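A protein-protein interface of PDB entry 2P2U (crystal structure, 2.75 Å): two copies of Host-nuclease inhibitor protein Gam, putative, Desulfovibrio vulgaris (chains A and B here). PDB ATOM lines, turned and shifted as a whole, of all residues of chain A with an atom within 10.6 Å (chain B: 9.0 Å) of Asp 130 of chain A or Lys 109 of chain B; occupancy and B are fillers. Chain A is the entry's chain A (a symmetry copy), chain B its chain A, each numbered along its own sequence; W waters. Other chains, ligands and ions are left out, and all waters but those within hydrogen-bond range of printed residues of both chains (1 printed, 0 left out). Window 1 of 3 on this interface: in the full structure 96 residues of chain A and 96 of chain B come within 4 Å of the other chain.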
ATOM      1  N   ILE A 127      15.999 -39.084   8.969  1.00  0.00           N
ATOM      2  CA  ILE A 127      14.900 -38.084   8.754  1.00  0.00           C
ATOM      3  C   ILE A 127      15.054 -37.450   7.384  1.00  0.00           C
ATOM      4  O   ILE A 127      16.134 -37.233   6.962  1.00  0.00           O
ATOM      5  CB  ILE A 127      14.930 -36.917   9.818  1.00  0.00           C
ATOM      6  CG1 ILE A 127      15.256 -37.449  11.209  1.00  0.00           C
ATOM      7  CG2 ILE A 127      13.592 -36.142   9.840  1.00  0.00           C
ATOM      8  CD1 ILE A 127      15.426 -36.409  12.403  1.00  0.00           C
ATOM      9  N   LYS A 128      13.973 -37.132   6.703  1.00  0.00           N
ATOM     10  CA  LYS A 128      14.072 -36.346   5.490  1.00  0.00           C
ATOM     11  C   LYS A 128      12.935 -35.364   5.505  1.00  0.00           C
ATOM     12  O   LYS A 128      11.787 -35.738   5.367  1.00  0.00           O
ATOM     13  CB  LYS A 128      14.105 -37.228   4.250  1.00  0.00           C
ATOM     14  CG  LYS A 128      13.912 -36.515   2.907  1.00  0.00           C
ATOM     15  CD  LYS A 128      12.433 -36.753   2.336  1.00  0.00           C
ATOM     16  CE  LYS A 128      12.276 -36.776   0.773  1.00  0.00           C
ATOM     17  NZ  LYS A 128      13.192 -37.827   0.166  1.00  0.00           N
ATOM     18  N   GLU A 129      13.262 -34.096   5.753  1.00  0.00           N
ATOM     19  CA  GLU A 129      12.255 -33.074   5.999  1.00  0.00           C
ATOM     20  C   GLU A 129      11.997 -32.279   4.753  1.00  0.00           C
ATOM     21  O   GLU A 129      12.850 -32.102   3.918  1.00  0.00           O
ATOM     22  CB  GLU A 129      12.683 -32.172   7.167  1.00  0.00           C
ATOM     23  CG  GLU A 129      12.333 -32.778   8.525  1.00  0.00           C
ATOM     24  CD  GLU A 129      12.919 -32.068   9.759  1.00  0.00           C
ATOM     25  OE1 GLU A 129      14.167 -32.035   9.845  1.00  0.00           O
ATOM     26  OE2 GLU A 129      12.155 -31.620  10.684  1.00  0.00           O
ATOM     27  N   ASP A 130      10.804 -31.763   4.595  1.00  0.00           N
ATOM     28  CA  ASP A 130      10.535 -31.050   3.387  1.00  0.00           C
ATOM     29  C   ASP A 130       9.513 -30.016   3.590  1.00  0.00           C
ATOM     30  O   ASP A 130       8.680 -30.187   4.427  1.00  0.00           O
ATOM     31  CB  ASP A 130       9.988 -32.013   2.407  1.00  0.00           C
ATOM     32  CG  ASP A 130      10.613 -31.855   1.114  1.00  0.00           C
ATOM     33  OD1 ASP A 130      11.889 -31.916   1.171  1.00  0.00           O
ATOM     34  OD2 ASP A 130       9.849 -31.659   0.095  1.00  0.00           O
ATOM     35  N   VAL A 131       9.526 -28.984   2.766  1.00  0.00           N
ATOM     36  CA  VAL A 131       8.635 -27.867   2.968  1.00  0.00           C
ATOM     37  C   VAL A 131       7.364 -28.221   2.336  1.00  0.00           C
ATOM     38  O   VAL A 131       7.344 -28.660   1.263  1.00  0.00           O
ATOM     39  CB  VAL A 131       9.157 -26.595   2.306  1.00  0.00           C
ATOM     40  CG1 VAL A 131       8.204 -25.448   2.493  1.00  0.00           C
ATOM     41  CG2 VAL A 131      10.522 -26.270   2.866  1.00  0.00           C
ATOM     42  N   ASN A 132       6.294 -27.982   3.027  1.00  0.00           N
ATOM     43  CA  ASN A 132       4.967 -28.259   2.574  1.00  0.00           C
ATOM     44  C   ASN A 132       4.437 -27.105   1.735  1.00  0.00           C
ATOM     45  O   ASN A 132       3.863 -26.148   2.279  1.00  0.00           O
ATOM     46  CB  ASN A 132       4.125 -28.398   3.853  1.00  0.00           C
ATOM     47  CG  ASN A 132       2.752 -28.968   3.604  1.00  0.00           C
ATOM     48  OD1 ASN A 132       2.346 -29.257   2.470  1.00  0.00           O
ATOM     49  ND2 ASN A 132       2.008 -29.132   4.694  1.00  0.00           N
ATOM     50  N   LYS A 133       4.582 -27.173   0.421  1.00  0.00           N
ATOM     51  CA  LYS A 133       4.164 -26.006  -0.366  1.00  0.00           C
ATOM     52  C   LYS A 133       2.669 -25.745  -0.406  1.00  0.00           C
ATOM     53  O   LYS A 133       2.222 -24.707  -0.868  1.00  0.00           O
ATOM     54  CB  LYS A 133       4.898 -25.834  -1.726  1.00  0.00           C
ATOM     55  CG  LYS A 133       4.729 -26.908  -2.869  1.00  0.00           C
ATOM     56  CD  LYS A 133       5.945 -26.860  -3.907  1.00  0.00           C
ATOM     57  CE  LYS A 133       5.547 -27.181  -5.364  1.00  0.00           C
ATOM     58  NZ  LYS A 133       4.563 -28.321  -5.565  1.00  0.00           N
ATOM     59  N   GLU A 134       1.892 -26.622   0.203  1.00  0.00           N
ATOM     60  CA  GLU A 134       0.450 -26.430   0.201  1.00  0.00           C
ATOM     61  C   GLU A 134      -0.150 -25.750   1.383  1.00  0.00           C
ATOM     62  O   GLU A 134      -1.192 -25.138   1.228  1.00  0.00           O
ATOM     63  CB  GLU A 134      -0.266 -27.733  -0.079  1.00  0.00           C
ATOM     64  CG  GLU A 134       0.261 -28.298  -1.388  1.00  0.00           C
ATOM     65  CD  GLU A 134      -0.141 -29.706  -1.613  1.00  0.00           C
ATOM     66  OE1 GLU A 134      -0.051 -30.520  -0.633  1.00  0.00           O
ATOM     67  OE2 GLU A 134      -0.559 -29.978  -2.770  1.00  0.00           O
ATOM     68  N   ALA A 135       0.445 -25.853   2.565  1.00  0.00           N
ATOM     69  CA  ALA A 135       0.018 -24.951   3.636  1.00  0.00           C
ATOM     70  C   ALA A 135       0.531 -23.560   3.282  1.00  0.00           C
ATOM     71  O   ALA A 135      -0.018 -22.568   3.715  1.00  0.00           O
ATOM     72  CB  ALA A 135       0.559 -25.379   4.936  1.00  0.00           C
ATOM     73  N   MET A 136       1.576 -23.507   2.463  1.00  0.00           N
ATOM     74  CA  MET A 136       2.193 -22.247   2.090  1.00  0.00           C
ATOM     75  C   MET A 136       1.174 -21.412   1.311  1.00  0.00           C
ATOM     76  O   MET A 136       0.732 -20.356   1.792  1.00  0.00           O
ATOM     77  CB  MET A 136       3.514 -22.447   1.303  1.00  0.00           C
ATOM     78  CG  MET A 136       4.746 -22.938   2.120  1.00  0.00           C
ATOM     79  SD  MET A 136       4.845 -22.249   3.961  1.00  0.00           S
ATOM     80  CE  MET A 136       6.377 -23.202   4.556  1.00  0.00           C
ATOM     81  N   VAL A 147       9.614 -16.702   6.524  1.00  0.00           N
ATOM     82  CA  VAL A 147      10.204 -17.998   6.387  1.00  0.00           C
ATOM     83  C   VAL A 147      11.062 -18.145   5.133  1.00  0.00           C
ATOM     84  O   VAL A 147      11.453 -19.276   4.763  1.00  0.00           O
ATOM     85  CB  VAL A 147       9.188 -19.067   6.419  1.00  0.00           C
ATOM     86  CG1 VAL A 147       8.406 -18.960   7.685  1.00  0.00           C
ATOM     87  CG2 VAL A 147       8.339 -18.980   5.255  1.00  0.00           C
ATOM     88  N   GLY A 148      11.369 -17.003   4.491  1.00  0.00           N
ATOM     89  CA  GLY A 148      12.285 -16.977   3.370  1.00  0.00           C
ATOM     90  C   GLY A 148      11.715 -17.412   2.056  1.00  0.00           C
ATOM     91  O   GLY A 148      12.445 -17.900   1.229  1.00  0.00           O
ATOM     92  N   LEU A 149      10.414 -17.198   1.850  1.00  0.00           N
ATOM     93  CA  LEU A 149       9.701 -17.677   0.652  1.00  0.00           C
ATOM     94  C   LEU A 149       8.997 -16.522  -0.129  1.00  0.00           C
ATOM     95  O   LEU A 149       8.492 -15.579   0.482  1.00  0.00           O
ATOM     96  CB  LEU A 149       8.657 -18.714   1.063  1.00  0.00           C
ATOM     97  CG  LEU A 149       9.195 -20.046   1.557  1.00  0.00           C
ATOM     98  CD1 LEU A 149       8.149 -21.005   2.018  1.00  0.00           C
ATOM     99  CD2 LEU A 149       9.999 -20.678   0.462  1.00  0.00           C
ATOM    100  N   VAL B 102       8.322 -19.930  -4.137  1.00  0.00           N
ATOM    101  CA  VAL B 102       9.721 -20.247  -4.408  1.00  0.00           C
ATOM    102  C   VAL B 102      10.688 -19.730  -3.307  1.00  0.00           C
ATOM    103  O   VAL B 102      10.275 -18.931  -2.459  1.00  0.00           O
ATOM    104  CB  VAL B 102      10.054 -19.738  -5.803  1.00  0.00           C
ATOM    105  CG1 VAL B 102      11.505 -19.972  -6.130  1.00  0.00           C
ATOM    106  CG2 VAL B 102       9.213 -20.508  -6.815  1.00  0.00           C
ATOM    107  N   GLN B 103      11.944 -20.169  -3.281  1.00  0.00           N
ATOM    108  CA  GLN B 103      12.864 -19.678  -2.234  1.00  0.00           C
ATOM    109  C   GLN B 103      13.181 -18.212  -2.445  1.00  0.00           C
ATOM    110  O   GLN B 103      13.270 -17.806  -3.571  1.00  0.00           O
ATOM    111  CB  GLN B 103      14.172 -20.481  -2.151  1.00  0.00           C
ATOM    112  CG  GLN B 103      14.034 -21.879  -1.634  1.00  0.00           C
ATOM    113  CD  GLN B 103      13.293 -21.974  -0.327  1.00  0.00           C
ATOM    114  OE1 GLN B 103      12.344 -22.768  -0.212  1.00  0.00           O
ATOM    115  NE2 GLN B 103      13.701 -21.165   0.684  1.00  0.00           N
ATOM    116  N   MET B 104      13.368 -17.414  -1.399  1.00  0.00           N
ATOM    117  CA  MET B 104      13.896 -16.080  -1.638  1.00  0.00           C
ATOM    118  C   MET B 104      15.329 -16.129  -2.089  1.00  0.00           C
ATOM    119  O   MET B 104      15.907 -17.217  -2.178  1.00  0.00           O
ATOM    120  CB  MET B 104      13.718 -15.183  -0.451  1.00  0.00           C
ATOM    121  CG  MET B 104      12.367 -14.569  -0.541  1.00  0.00           C
ATOM    122  SD  MET B 104      11.879 -13.553   1.034  1.00  0.00           S
ATOM    123  CE  MET B 104      13.284 -12.116   0.965  1.00  0.00           C
ATOM    124  N   SER B 105      15.919 -14.979  -2.396  1.00  0.00           N
ATOM    125  CA  SER B 105      17.200 -15.057  -3.111  1.00  0.00           C
ATOM    126  C   SER B 105      18.308 -15.791  -2.348  1.00  0.00           C
ATOM    127  O   SER B 105      18.904 -16.710  -2.926  1.00  0.00           O
ATOM    128  CB  SER B 105      17.694 -13.718  -3.686  1.00  0.00           C
ATOM    129  OG  SER B 105      17.284 -12.593  -2.862  1.00  0.00           O
ATOM    130  N   LYS B 106      18.655 -15.450  -1.106  1.00  0.00           N
ATOM    131  CA  LYS B 106      19.854 -16.187  -0.703  1.00  0.00           C
ATOM    132  C   LYS B 106      19.581 -17.275   0.301  1.00  0.00           C
ATOM    133  O   LYS B 106      20.468 -17.604   1.094  1.00  0.00           O
ATOM    134  CB  LYS B 106      20.957 -15.262  -0.227  1.00  0.00           C
ATOM    135  CG  LYS B 106      21.068 -13.943  -1.005  1.00  0.00           C
ATOM    136  CD  LYS B 106      21.748 -12.888  -0.185  1.00  0.00           C
ATOM    137  CE  LYS B 106      20.936 -11.598  -0.195  1.00  0.00           C
ATOM    138  NZ  LYS B 106      21.745 -10.548   0.480  1.00  0.00           N
ATOM    139  N   ILE B 107      18.363 -17.833   0.252  1.00  0.00           N
ATOM    140  CA  ILE B 107      17.828 -18.666   1.291  1.00  0.00           C
ATOM    141  C   ILE B 107      17.561 -20.100   0.802  1.00  0.00           C
ATOM    142  O   ILE B 107      16.692 -20.339   0.016  1.00  0.00           O
ATOM    143  CB  ILE B 107      16.455 -18.121   1.757  1.00  0.00           C
ATOM    144  CG1 ILE B 107      16.446 -16.596   1.954  1.00  0.00           C
ATOM    145  CG2 ILE B 107      15.900 -18.911   2.978  1.00  0.00           C
ATOM    146  CD1 ILE B 107      16.988 -16.061   3.191  1.00  0.00           C
ATOM    147  N   THR B 108      18.249 -21.071   1.335  1.00  0.00           N
ATOM    148  CA  THR B 108      18.036 -22.417   0.899  1.00  0.00           C
ATOM    149  C   THR B 108      16.795 -22.950   1.503  1.00  0.00           C
ATOM    150  O   THR B 108      16.348 -22.465   2.491  1.00  0.00           O
ATOM    151  CB  THR B 108      19.142 -23.319   1.415  1.00  0.00           C
ATOM    152  OG1 THR B 108      19.177 -23.174   2.852  1.00  0.00           O
ATOM    153  CG2 THR B 108      20.452 -22.972   0.817  1.00  0.00           C
ATOM    154  N   LYS B 109      16.285 -24.035   0.943  1.00  0.00           N
ATOM    155  CA  LYS B 109      15.096 -24.713   1.475  1.00  0.00           C
ATOM    156  C   LYS B 109      15.316 -25.291   2.892  1.00  0.00           C
ATOM    157  O   LYS B 109      14.389 -25.357   3.691  1.00  0.00           O
ATOM    158  CB  LYS B 109      14.600 -25.743   0.434  1.00  0.00           C
ATOM    159  CG  LYS B 109      13.910 -26.987   0.981  1.00  0.00           C
ATOM    160  CD  LYS B 109      13.120 -27.694  -0.130  1.00  0.00           C
ATOM    161  CE  LYS B 109      11.982 -28.647   0.395  1.00  0.00           C
ATOM    162  NZ  LYS B 109      11.462 -29.342  -0.860  1.00  0.00           N
ATOM    163  N   ASP B 110      16.524 -25.687   3.240  1.00  0.00           N
ATOM    164  CA  ASP B 110      16.798 -26.068   4.624  1.00  0.00           C
ATOM    165  C   ASP B 110      16.758 -24.846   5.591  1.00  0.00           C
ATOM    166  O   ASP B 110      16.500 -25.017   6.797  1.00  0.00           O
ATOM    167  CB  ASP B 110      18.174 -26.654   4.748  1.00  0.00           C
ATOM    168  CG  ASP B 110      18.288 -28.129   4.388  1.00  0.00           C
ATOM    169  OD1 ASP B 110      17.273 -28.872   4.219  1.00  0.00           O
ATOM    170  OD2 ASP B 110      19.482 -28.547   4.327  1.00  0.00           O
ATOM    171  N   MET B 111      17.047 -23.625   5.123  1.00  0.00           N
ATOM    172  CA  MET B 111      16.924 -22.508   6.051  1.00  0.00           C
ATOM    173  C   MET B 111      15.459 -22.142   6.298  1.00  0.00           C
ATOM    174  O   MET B 111      15.084 -21.737   7.407  1.00  0.00           O
ATOM    175  CB  MET B 111      17.763 -21.331   5.632  1.00  0.00           C
ATOM    176  CG  MET B 111      19.235 -21.687   5.403  1.00  0.00           C
ATOM    177  SD  MET B 111      20.151 -20.320   4.237  1.00  0.00           S
ATOM    178  CE  MET B 111      19.365 -18.713   5.130  1.00  0.00           C
ATOM    179  N   THR B 112      14.625 -22.319   5.286  1.00  0.00           N
ATOM    180  CA  THR B 112      13.185 -22.166   5.443  1.00  0.00           C
ATOM    181  C   THR B 112      12.600 -23.174   6.432  1.00  0.00           C
ATOM    182  O   THR B 112      11.748 -22.810   7.302  1.00  0.00           O
ATOM    183  CB  THR B 112      12.553 -22.290   4.121  1.00  0.00           C
ATOM    184  OG1 THR B 112      12.920 -21.110   3.397  1.00  0.00           O
ATOM    185  CG2 THR B 112      11.040 -22.395   4.162  1.00  0.00           C
ATOM    186  N   LEU B 113      13.051 -24.435   6.348  1.00  0.00           N
ATOM    187  CA  LEU B 113      12.646 -25.419   7.382  1.00  0.00           C
ATOM    188  C   LEU B 113      12.999 -25.016   8.816  1.00  0.00           C
ATOM    189  O   LEU B 113      12.228 -25.254   9.719  1.00  0.00           O
ATOM    190  CB  LEU B 113      13.301 -26.774   7.123  1.00  0.00           C
ATOM    191  CG  LEU B 113      12.632 -27.331   5.878  1.00  0.00           C
ATOM    192  CD1 LEU B 113      13.294 -28.573   5.320  1.00  0.00           C
ATOM    193  CD2 LEU B 113      11.149 -27.615   6.182  1.00  0.00           C
ATOM    194  N   GLU B 114      14.204 -24.503   9.019  1.00  0.00           N
ATOM    195  CA  GLU B 114      14.655 -24.295  10.351  1.00  0.00           C
ATOM    196  C   GLU B 114      13.862 -23.114  10.818  1.00  0.00           C
ATOM    197  O   GLU B 114      13.451 -23.023  11.975  1.00  0.00           O
ATOM    198  CB  GLU B 114      16.180 -24.121  10.414  1.00  0.00           C
ATOM    199  CG  GLU B 114      16.767 -23.886  11.817  1.00  0.00           C
ATOM    200  CD  GLU B 114      16.153 -24.776  12.950  1.00  0.00           C
ATOM    201  OE1 GLU B 114      15.910 -24.246  14.077  1.00  0.00           O
ATOM    202  OE2 GLU B 114      15.898 -25.984  12.687  1.00  0.00           O
ATOM    203  N   ARG B 115      13.580 -22.187   9.913  1.00  0.00           N
ATOM    204  CA  ARG B 115      12.722 -21.143  10.350  1.00  0.00           C
ATOM    205  C   ARG B 115      11.394 -21.563  10.653  1.00  0.00           C
ATOM    206  O   ARG B 115      10.862 -21.018  11.591  1.00  0.00           O
ATOM    207  CB  ARG B 115      12.506 -20.144   9.308  1.00  0.00           C
ATOM    208  CG  ARG B 115      13.689 -19.361   9.132  1.00  0.00           C
ATOM    209  CD  ARG B 115      13.438 -18.243   8.153  1.00  0.00           C
ATOM    210  NE  ARG B 115      14.739 -17.602   7.767  1.00  0.00           N
ATOM    211  CZ  ARG B 115      14.951 -16.450   7.001  1.00  0.00           C
ATOM    212  NH1 ARG B 115      13.958 -15.726   6.476  1.00  0.00           N
ATOM    213  NH2 ARG B 115      16.167 -15.969   6.715  1.00  0.00           N
ATOM    214  N   LEU B 116      10.780 -22.404   9.809  1.00  0.00           N
ATOM    215  CA  LEU B 116       9.428 -22.898  10.120  1.00  0.00           C
ATOM    216  C   LEU B 116       9.470 -23.458  11.516  1.00  0.00           C
ATOM    217  O   LEU B 116       8.501 -23.351  12.242  1.00  0.00           O
ATOM    218  CB  LEU B 116       8.926 -23.901   9.075  1.00  0.00           C
ATOM    219  CG  LEU B 116       8.436 -23.092   7.831  1.00  0.00           C
ATOM    220  CD1 LEU B 116       8.497 -23.895   6.562  1.00  0.00           C
ATOM    221  CD2 LEU B 116       7.058 -22.526   8.079  1.00  0.00           C
ATOM    222  N   ARG B 117      10.613 -23.958  11.947  1.00  0.00           N
ATOM    223  CA  ARG B 117      10.653 -24.781  13.114  1.00  0.00           C
ATOM    224  C   ARG B 117      10.908 -23.831  14.301  1.00  0.00           C
ATOM    225  O   ARG B 117      10.228 -23.920  15.315  1.00  0.00           O
ATOM    226  CB  ARG B 117      11.701 -25.852  12.872  1.00  0.00           C
ATOM    227  CG  ARG B 117      11.867 -26.963  13.901  1.00  0.00           C
ATOM    228  CD  ARG B 117      13.212 -27.858  13.651  1.00  0.00           C
ATOM    229  NE  ARG B 117      13.111 -28.701  12.438  1.00  0.00           N
ATOM    230  CZ  ARG B 117      13.914 -28.589  11.361  1.00  0.00           C
ATOM    231  NH1 ARG B 117      13.718 -29.340  10.287  1.00  0.00           N
ATOM    232  NH2 ARG B 117      14.921 -27.720  11.323  1.00  0.00           N
ATOM    233  N   ILE B 121       5.976 -23.828  13.398  1.00  0.00           N
ATOM    234  CA  ILE B 121       4.971 -24.079  12.400  1.00  0.00           C
ATOM    235  C   ILE B 121       5.196 -25.495  11.939  1.00  0.00           C
ATOM    236  O   ILE B 121       5.986 -25.741  11.048  1.00  0.00           O
ATOM    237  CB  ILE B 121       5.100 -23.127  11.138  1.00  0.00           C
ATOM    238  CG1 ILE B 121       4.988 -21.676  11.515  1.00  0.00           C
ATOM    239  CG2 ILE B 121       4.024 -23.416  10.162  1.00  0.00           C
ATOM    240  CD1 ILE B 121       3.697 -21.365  12.182  1.00  0.00           C
ATOM    241  N   SER B 122       4.488 -26.454  12.513  1.00  0.00           N
ATOM    242  CA  SER B 122       4.720 -27.834  12.047  1.00  0.00           C
ATOM    243  C   SER B 122       3.913 -28.185  10.823  1.00  0.00           C
ATOM    244  O   SER B 122       4.350 -29.056  10.089  1.00  0.00           O
ATOM    245  CB  SER B 122       4.542 -28.840  13.136  1.00  0.00           C
ATOM    246  OG  SER B 122       3.167 -28.854  13.434  1.00  0.00           O
ATOM    247  N   GLU B 123       2.780 -27.517  10.571  1.00  0.00           N
ATOM    248  CA  GLU B 123       2.043 -27.626   9.261  1.00  0.00           C
ATOM    249  C   GLU B 123       2.877 -27.266   8.025  1.00  0.00           C
ATOM    250  O   GLU B 123       2.574 -27.704   6.920  1.00  0.00           O
ATOM    251  CB  GLU B 123       0.760 -26.758   9.218  1.00  0.00           C
ATOM    252  CG  GLU B 123       0.820 -25.386   9.896  1.00  0.00           C
ATOM    253  CD  GLU B 123       0.740 -25.500  11.435  1.00  0.00           C
ATOM    254  OE1 GLU B 123       1.644 -26.095  12.084  1.00  0.00           O
ATOM    255  OE2 GLU B 123      -0.250 -25.008  12.019  1.00  0.00           O
ATOM    256  N   GLY B 124       3.916 -26.462   8.210  1.00  0.00           N
ATOM    257  CA  GLY B 124       4.763 -26.166   7.110  1.00  0.00           C
ATOM    258  C   GLY B 124       5.710 -27.273   6.685  1.00  0.00           C
ATOM    259  O   GLY B 124       6.337 -27.171   5.610  1.00  0.00           O
ATOM    260  N   ILE B 125       5.847 -28.315   7.520  1.00  0.00           N
ATOM    261  CA  ILE B 125       6.942 -29.283   7.361  1.00  0.00           C
ATOM    262  C   ILE B 125       6.481 -30.688   6.977  1.00  0.00           C
ATOM    263  O   ILE B 125       5.585 -31.229   7.571  1.00  0.00           O
ATOM    264  CB  ILE B 125       7.868 -29.281   8.606  1.00  0.00           C
ATOM    265  CG1 ILE B 125       8.491 -27.914   8.759  1.00  0.00           C
ATOM    266  CG2 ILE B 125       9.046 -30.175   8.412  1.00  0.00           C
ATOM    267  CD1 ILE B 125       9.042 -27.583  10.106  1.00  0.00           C
ATOM    268  N   ARG B 126       7.099 -31.288   5.980  1.00  0.00           N
ATOM    269  CA  ARG B 126       6.812 -32.683   5.643  1.00  0.00           C
ATOM    270  C   ARG B 126       7.924 -33.658   6.069  1.00  0.00           C
ATOM    271  O   ARG B 126       9.035 -33.516   5.607  1.00  0.00           O
ATOM    272  CB  ARG B 126       6.594 -32.790   4.136  1.00  0.00           C
ATOM    273  CG  ARG B 126       5.184 -32.627   3.698  1.00  0.00           C
ATOM    274  CD  ARG B 126       5.152 -32.126   2.239  1.00  0.00           C
ATOM    275  NE  ARG B 126       3.961 -32.620   1.541  1.00  0.00           N
ATOM    276  CZ  ARG B 126       2.691 -32.448   1.955  1.00  0.00           C
ATOM    277  NH1 ARG B 126       2.389 -31.776   3.057  1.00  0.00           N
ATOM    278  NH2 ARG B 126       1.698 -32.962   1.256  1.00  0.00           N
ATOM    279  N   ILE B 127       7.641 -34.661   6.901  1.00  0.00           N
ATOM    280  CA  ILE B 127       8.728 -35.499   7.507  1.00  0.00           C
ATOM    281  C   ILE B 127       8.632 -36.916   6.971  1.00  0.00           C
ATOM    282  O   ILE B 127       7.570 -37.390   6.768  1.00  0.00           O
ATOM    283  CB  ILE B 127       8.619 -35.584   9.081  1.00  0.00           C
ATOM    284  CG1 ILE B 127       8.233 -34.236   9.678  1.00  0.00           C
ATOM    285  CG2 ILE B 127       9.937 -36.093   9.710  1.00  0.00           C
ATOM    286  CD1 ILE B 127       7.980 -34.142  11.248  1.00  0.00           C
ATOM    287  N   LYS B 128       9.739 -37.598   6.766  1.00  0.00           N
ATOM    288  CA  LYS B 128       9.686 -39.011   6.451  1.00  0.00           C
ATOM    289  C   LYS B 128      10.800 -39.676   7.210  1.00  0.00           C
ATOM    290  O   LYS B 128      11.961 -39.482   6.909  1.00  0.00           O
ATOM    291  CB  LYS B 128       9.736 -39.254   4.950  1.00  0.00           C
ATOM    292  CG  LYS B 128       9.983 -40.701   4.506  1.00  0.00           C
ATOM    293  CD  LYS B 128      11.494 -40.900   4.010  1.00  0.00           C
ATOM    294  CE  LYS B 128      11.732 -41.978   2.891  1.00  0.00           C
ATOM    295  NZ  LYS B 128      10.872 -41.675   1.675  1.00  0.00           N
HETATM  296  O   HOH W   1       9.523 -35.572   3.078  1.00  0.00           O
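NH1 of Arg 117 of chain B lies within salt-bridge range of OE1 of Glu 129 of chain A. The guanidinium group (NH1) of Arg 126 of chain B lies within hydrogen-bond range of the side-chain amide oxygen (OD1) of Asn 132 of chain A, 2.6 Å away. The side-chain amide nitrogen (ND2) of Asn 132 of chain A sits at hydrogen-bond distance from the backbone carbonyl oxygen (O) of Glu 123 of chain B (2.7 Å). The guanidinium group (NH2) of Arg 126 of chain B is in salt-bridge range of the side-chain carboxylate (OE1) of Glu 134 of chain A (3.5 Å). The backbone carbonyl oxygen (O) of Gly 124 of chain B lies within hydrogen-bond range of the backbone NH (N) of Asn 132 of chain A. The backbone NH (N) of Met 104 of chain B is in hydrogen-bond range of the backbone carbonyl oxygen (O) of Gly 148 of chain A (2.8 Å). The backbone NH of Lys 128 of chain B is in hydrogen-bond range of the backbone carbonyl oxygen of Lys 128 of chain A, 3.1 Å away. The backbone carbonyl oxygen (O) of Val 147 of chain A is in hydrogen-bond range of the side-chain hydroxyl (OG1) of Thr 112 of chain B (2.7 Å). The side-chain carboxylate of Asp 130 of chain A lies within salt-bridge range of the side-chain amino group of Lys 109 of chain B. The backbone NH (N) of Arg 126 of chain B sits at hydrogen-bond distance from the backbone carbonyl oxygen (O) of Asp 130 of chain A.
The side-chain amide nitrogen (NE2) of Gln 103 of chain B is in hydrogen-bond range of the backbone carbonyl oxygen (O) of Ile 107 of chain B. OG1 of Thr 112 of chain B lies within hydrogen-bond range of NE2 of Gln 103 of chain B (2.8 Å).
Lys 109 of chain B touches just these residues of chain A: Asp 130 and Val 131. No residue of chain A comes within 4 Å of Thr 108 of chain B. No residue of chain A comes within 4 Å of Asp 110 of chain B. Printed residues of chain A within 4 Å of Gln 103 of chain B: Gly 148 (3.5 Å) and Leu 149 (3.2 Å). Ile 121 of chain B touches none of the printed residues of chain A. The nearest printed residue of chain B that does not touch Asp 130 of chain A is Ile 127 of chain B (4.9 Å). The nearest printed residue of chain B that does not touch Asn 132 of chain A is Ile 125 of chain B (4.1 Å).
Of the 24 printed residues of chain B, 15 touch a printed residue of chain A. Hydrophobic or aromatic side chains of chain B within 4 Å of the printed part of chain A: Met 104, Leu 113, Leu 116 and Ile 127. Of the 13 printed residues of chain A, 12 touch a printed residue of chain B.
Lys 128 of chain B touches its own counterpart, Lys 128 of chain A. Of the 33 pairs that touch across the chains among the printed residues, 4 have their exchanged pair printed and touching as well.
Water W1 lies within hydrogen-bond range of O of Lys 128 of chain A and O of Arg 126 of chain B.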
